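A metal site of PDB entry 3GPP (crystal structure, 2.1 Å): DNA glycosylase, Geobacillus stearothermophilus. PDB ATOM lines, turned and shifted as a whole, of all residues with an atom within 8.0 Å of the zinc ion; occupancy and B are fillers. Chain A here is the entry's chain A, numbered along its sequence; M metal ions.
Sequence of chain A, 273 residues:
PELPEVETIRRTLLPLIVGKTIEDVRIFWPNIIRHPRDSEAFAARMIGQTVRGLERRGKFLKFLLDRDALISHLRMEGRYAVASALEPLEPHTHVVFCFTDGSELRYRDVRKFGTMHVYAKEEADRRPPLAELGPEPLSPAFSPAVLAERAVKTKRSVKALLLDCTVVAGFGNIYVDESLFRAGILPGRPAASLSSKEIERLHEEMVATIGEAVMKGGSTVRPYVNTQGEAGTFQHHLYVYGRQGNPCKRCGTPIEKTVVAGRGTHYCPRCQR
N of Arg 250 sits close to SG of Cys 248 (3.3 Å).
N of Arg 270 sits close to SG of Cys 268 (3.5 Å).
SG of Cys 251 sits close to OG1 of Thr 253.
The backbone carbonyl oxygen (O) of Thr 253 lies within hydrogen-bond range of the backbone NH (N) of Cys 248.
OE1 of Gln 272 lies within hydrogen-bond range of N of Cys 268, at 2.9 Å.
Within 4 Å of the zinc ion: Cys 248, Cys 251, Cys 268 and Cys 271.
Along chain A the residues within 4 Å of the zinc ion span positions 248 to 271.
The nearest printed residue that does not touch the zinc ion is Phe 181 (4.2 Å).
The zinc ion is bound by the side-chain sulfur of Cys 271, the side-chain sulfur of Cys 268, the side-chain sulfur of Cys 251 and the side-chain sulfur of Cys 248.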
ATOM      1  N   PHE A 181       3.748  23.757   6.226  1.00  0.00           N
ATOM      2  CA  PHE A 181       4.388  22.654   5.525  1.00  0.00           C
ATOM      3  C   PHE A 181       4.063  22.690   4.018  1.00  0.00           C
ATOM      4  O   PHE A 181       4.952  22.702   3.192  1.00  0.00           O
ATOM      5  CB  PHE A 181       4.024  21.271   6.093  1.00  0.00           C
ATOM      6  CG  PHE A 181       4.463  20.162   5.206  1.00  0.00           C
ATOM      7  CD1 PHE A 181       5.787  19.702   5.253  1.00  0.00           C
ATOM      8  CD2 PHE A 181       3.608  19.629   4.231  1.00  0.00           C
ATOM      9  CE1 PHE A 181       6.225  18.678   4.399  1.00  0.00           C
ATOM     10  CE2 PHE A 181       4.040  18.632   3.364  1.00  0.00           C
ATOM     11  CZ  PHE A 181       5.347  18.141   3.447  1.00  0.00           C
ATOM     12  N   TYR A 239       0.408  15.895   7.196  1.00  0.00           N
ATOM     13  CA  TYR A 239       1.797  15.816   6.741  1.00  0.00           C
ATOM     14  C   TYR A 239       2.799  15.913   7.889  1.00  0.00           C
ATOM     15  O   TYR A 239       3.851  15.276   7.830  1.00  0.00           O
ATOM     16  CB  TYR A 239       2.084  16.932   5.730  1.00  0.00           C
ATOM     17  CG  TYR A 239       1.410  16.734   4.398  1.00  0.00           C
ATOM     18  CD1 TYR A 239       0.332  17.537   4.026  1.00  0.00           C
ATOM     19  CD2 TYR A 239       1.852  15.760   3.503  1.00  0.00           C
ATOM     20  CE1 TYR A 239      -0.292  17.365   2.796  1.00  0.00           C
ATOM     21  CE2 TYR A 239       1.220  15.570   2.269  1.00  0.00           C
ATOM     22  CZ  TYR A 239       0.149  16.385   1.932  1.00  0.00           C
ATOM     23  OH  TYR A 239      -0.486  16.204   0.719  1.00  0.00           O
ATOM     24  N   VAL A 240       2.495  16.734   8.903  1.00  0.00           N
ATOM     25  CA  VAL A 240       3.476  17.023   9.961  1.00  0.00           C
ATOM     26  C   VAL A 240       2.963  16.927  11.402  1.00  0.00           C
ATOM     27  O   VAL A 240       3.695  16.468  12.293  1.00  0.00           O
ATOM     28  CB  VAL A 240       4.206  18.415   9.761  1.00  0.00           C
ATOM     29  CG1 VAL A 240       5.058  18.387   8.489  1.00  0.00           C
ATOM     30  CG2 VAL A 240       3.211  19.607   9.761  1.00  0.00           C
ATOM     31  N   PRO A 247       8.873   9.715   8.952  1.00  0.00           N
ATOM     32  CA  PRO A 247       9.298  10.275   7.666  1.00  0.00           C
ATOM     33  C   PRO A 247       8.271  11.232   7.039  1.00  0.00           C
ATOM     34  O   PRO A 247       7.054  10.984   7.095  1.00  0.00           O
ATOM     35  CB  PRO A 247       9.504   9.041   6.783  1.00  0.00           C
ATOM     36  CG  PRO A 247       8.760   7.944   7.457  1.00  0.00           C
ATOM     37  CD  PRO A 247       8.708   8.253   8.912  1.00  0.00           C
ATOM     38  N   CYS A 248       8.769  12.333   6.503  1.00  0.00           N
ATOM     39  CA  CYS A 248       7.987  13.230   5.684  1.00  0.00           C
ATOM     40  C   CYS A 248       7.403  12.458   4.503  1.00  0.00           C
ATOM     41  O   CYS A 248       8.126  11.731   3.802  1.00  0.00           O
ATOM     42  CB  CYS A 248       8.866  14.361   5.152  1.00  0.00           C
ATOM     43  SG  CYS A 248       7.951  15.467   4.078  1.00  0.00           S
ATOM     44  N   LYS A 249       6.107  12.628   4.304  1.00  0.00           N
ATOM     45  CA  LYS A 249       5.365  12.003   3.229  1.00  0.00           C
ATOM     46  C   LYS A 249       5.809  12.483   1.832  1.00  0.00           C
ATOM     47  O   LYS A 249       5.472  11.851   0.843  1.00  0.00           O
ATOM     48  CB  LYS A 249       3.860  12.241   3.403  1.00  0.00           C
ATOM     49  CG  LYS A 249       3.302  11.695   4.717  1.00  0.00           C
ATOM     50  CD  LYS A 249       1.781  11.729   4.756  1.00  0.00           C
ATOM     51  CE  LYS A 249       1.259  11.089   6.061  1.00  0.00           C
ATOM     52  NZ  LYS A 249      -0.190  10.713   6.005  1.00  0.00           N
ATOM     53  N   ARG A 250       6.550  13.587   1.770  1.00  0.00           N
ATOM     54  CA  ARG A 250       6.995  14.106   0.469  1.00  0.00           C
ATOM     55  C   ARG A 250       8.482  13.882   0.194  1.00  0.00           C
ATOM     56  O   ARG A 250       8.873  13.796  -0.962  1.00  0.00           O
ATOM     57  CB  ARG A 250       6.650  15.598   0.314  1.00  0.00           C
ATOM     58  CG  ARG A 250       5.151  15.874   0.322  1.00  0.00           C
ATOM     59  CD  ARG A 250       4.783  16.938  -0.723  1.00  0.00           C
ATOM     60  NE  ARG A 250       3.335  17.104  -0.869  1.00  0.00           N
ATOM     61  CZ  ARG A 250       2.657  18.211  -0.540  1.00  0.00           C
ATOM     62  NH1 ARG A 250       1.342  18.251  -0.715  1.00  0.00           N
ATOM     63  NH2 ARG A 250       3.279  19.272  -0.030  1.00  0.00           N
ATOM     64  N   CYS A 251       9.317  13.811   1.220  1.00  0.00           N
ATOM     65  CA  CYS A 251      10.748  13.716   1.001  1.00  0.00           C
ATOM     66  C   CYS A 251      11.415  12.654   1.863  1.00  0.00           C
ATOM     67  O   CYS A 251      12.572  12.340   1.654  1.00  0.00           O
ATOM     68  CB  CYS A 251      11.435  15.072   1.188  1.00  0.00           C
ATOM     69  SG  CYS A 251      11.666  15.512   2.921  1.00  0.00           S
ATOM     70  N   GLY A 252      10.665  12.094   2.816  1.00  0.00           N
ATOM     71  CA  GLY A 252      11.171  11.010   3.664  1.00  0.00           C
ATOM     72  C   GLY A 252      12.058  11.464   4.809  1.00  0.00           C
ATOM     73  O   GLY A 252      12.576  10.627   5.559  1.00  0.00           O
ATOM     74  N   THR A 253      12.261  12.777   4.956  1.00  0.00           N
ATOM     75  CA  THR A 253      13.028  13.326   6.081  1.00  0.00           C
ATOM     76  C   THR A 253      12.206  13.223   7.373  1.00  0.00           C
ATOM     77  O   THR A 253      11.018  13.543   7.371  1.00  0.00           O
ATOM     78  CB  THR A 253      13.425  14.795   5.831  1.00  0.00           C
ATOM     79  OG1 THR A 253      14.220  14.869   4.645  1.00  0.00           O
ATOM     80  CG2 THR A 253      14.221  15.388   7.009  1.00  0.00           C
ATOM     81  N   PRO A 254      12.844  12.771   8.485  1.00  0.00           N
ATOM     82  CA  PRO A 254      12.101  12.749   9.742  1.00  0.00           C
ATOM     83  C   PRO A 254      11.530  14.128  10.080  1.00  0.00           C
ATOM     84  O   PRO A 254      12.252  15.129  10.021  1.00  0.00           O
ATOM     85  CB  PRO A 254      13.157  12.323  10.776  1.00  0.00           C
ATOM     86  CG  PRO A 254      14.184  11.601   9.989  1.00  0.00           C
ATOM     87  CD  PRO A 254      14.223  12.265   8.646  1.00  0.00           C
ATOM     88  N   ILE A 255      10.251  14.149  10.434  1.00  0.00           N
ATOM     89  CA  ILE A 255       9.591  15.362  10.877  1.00  0.00           C
ATOM     90  C   ILE A 255      10.146  15.734  12.244  1.00  0.00           C
ATOM     91  O   ILE A 255      10.374  14.861  13.095  1.00  0.00           O
ATOM     92  CB  ILE A 255       8.060  15.173  10.942  1.00  0.00           C
ATOM     93  CG1 ILE A 255       7.488  14.895   9.527  1.00  0.00           C
ATOM     94  CG2 ILE A 255       7.360  16.374  11.624  1.00  0.00           C
ATOM     95  CD1 ILE A 255       7.988  15.882   8.419  1.00  0.00           C
ATOM     96  N   TYR A 267       7.383  20.317  11.780  1.00  0.00           N
ATOM     97  CA  TYR A 267       7.885  20.742  10.477  1.00  0.00           C
ATOM     98  C   TYR A 267       8.830  19.719   9.838  1.00  0.00           C
ATOM     99  O   TYR A 267       9.444  18.882  10.515  1.00  0.00           O
ATOM    100  CB  TYR A 267       8.560  22.139  10.586  1.00  0.00           C
ATOM    101  CG  TYR A 267       9.810  22.136  11.437  1.00  0.00           C
ATOM    102  CD1 TYR A 267      11.073  22.005  10.853  1.00  0.00           C
ATOM    103  CD2 TYR A 267       9.744  22.249  12.832  1.00  0.00           C
ATOM    104  CE1 TYR A 267      12.221  21.985  11.627  1.00  0.00           C
ATOM    105  CE2 TYR A 267      10.880  22.233  13.613  1.00  0.00           C
ATOM    106  CZ  TYR A 267      12.121  22.094  13.011  1.00  0.00           C
ATOM    107  OH  TYR A 267      13.269  22.096  13.785  1.00  0.00           O
ATOM    108  N   CYS A 268       8.919  19.783   8.516  1.00  0.00           N
ATOM    109  CA  CYS A 268       9.971  19.096   7.780  1.00  0.00           C
ATOM    110  C   CYS A 268      11.077  20.112   7.483  1.00  0.00           C
ATOM    111  O   CYS A 268      10.847  21.105   6.791  1.00  0.00           O
ATOM    112  CB  CYS A 268       9.434  18.490   6.480  1.00  0.00           C
ATOM    113  SG  CYS A 268      10.774  17.757   5.483  1.00  0.00           S
ATOM    114  N   PRO A 269      12.302  19.867   7.985  1.00  0.00           N
ATOM    115  CA  PRO A 269      13.377  20.832   7.804  1.00  0.00           C
ATOM    116  C   PRO A 269      13.966  20.821   6.388  1.00  0.00           C
ATOM    117  O   PRO A 269      14.884  21.600   6.098  1.00  0.00           O
ATOM    118  CB  PRO A 269      14.437  20.336   8.786  1.00  0.00           C
ATOM    119  CG  PRO A 269      14.278  18.874   8.726  1.00  0.00           C
ATOM    120  CD  PRO A 269      12.792  18.641   8.658  1.00  0.00           C
ATOM    121  N   ARG A 270      13.485  19.924   5.516  1.00  0.00           N
ATOM    122  CA  ARG A 270      13.928  19.921   4.124  1.00  0.00           C
ATOM    123  C   ARG A 270      12.900  20.591   3.219  1.00  0.00           C
ATOM    124  O   ARG A 270      13.245  21.423   2.394  1.00  0.00           O
ATOM    125  CB  ARG A 270      14.214  18.504   3.625  1.00  0.00           C
ATOM    126  CG  ARG A 270      14.740  18.456   2.198  1.00  0.00           C
ATOM    127  CD  ARG A 270      14.781  17.041   1.584  1.00  0.00           C
ATOM    128  NE  ARG A 270      15.288  17.105   0.215  1.00  0.00           N
ATOM    129  CZ  ARG A 270      15.783  16.079  -0.461  1.00  0.00           C
ATOM    130  NH1 ARG A 270      16.249  16.275  -1.706  1.00  0.00           N
ATOM    131  NH2 ARG A 270      15.824  14.865   0.089  1.00  0.00           N
ATOM    132  N   CYS A 271      11.633  20.185   3.351  1.00  0.00           N
ATOM    133  CA  CYS A 271      10.556  20.738   2.544  1.00  0.00           C
ATOM    134  C   CYS A 271      10.305  22.224   2.875  1.00  0.00           C
ATOM    135  O   CYS A 271       9.967  23.000   1.986  1.00  0.00           O
ATOM    136  CB  CYS A 271       9.266  19.912   2.706  1.00  0.00           C
ATOM    137  SG  CYS A 271       9.310  18.208   1.941  1.00  0.00           S
ATOM    138  N   GLN A 272      10.477  22.607   4.133  1.00  0.00           N
ATOM    139  CA  GLN A 272      10.166  23.967   4.580  1.00  0.00           C
ATOM    140  C   GLN A 272      11.414  24.839   4.721  1.00  0.00           C
ATOM    141  O   GLN A 272      12.414  24.379   5.271  1.00  0.00           O
ATOM    142  CB  GLN A 272       9.395  23.949   5.891  1.00  0.00           C
ATOM    143  CG  GLN A 272       8.040  23.332   5.737  1.00  0.00           C
ATOM    144  CD  GLN A 272       7.359  23.059   7.044  1.00  0.00           C
ATOM    145  OE1 GLN A 272       7.265  21.910   7.465  1.00  0.00           O
ATOM    146  NE2 GLN A 272       6.865  24.113   7.690  1.00  0.00           N
HETATM  147 ZN    ZN M   1       9.868  16.846   3.598  1.00  0.00          ZN
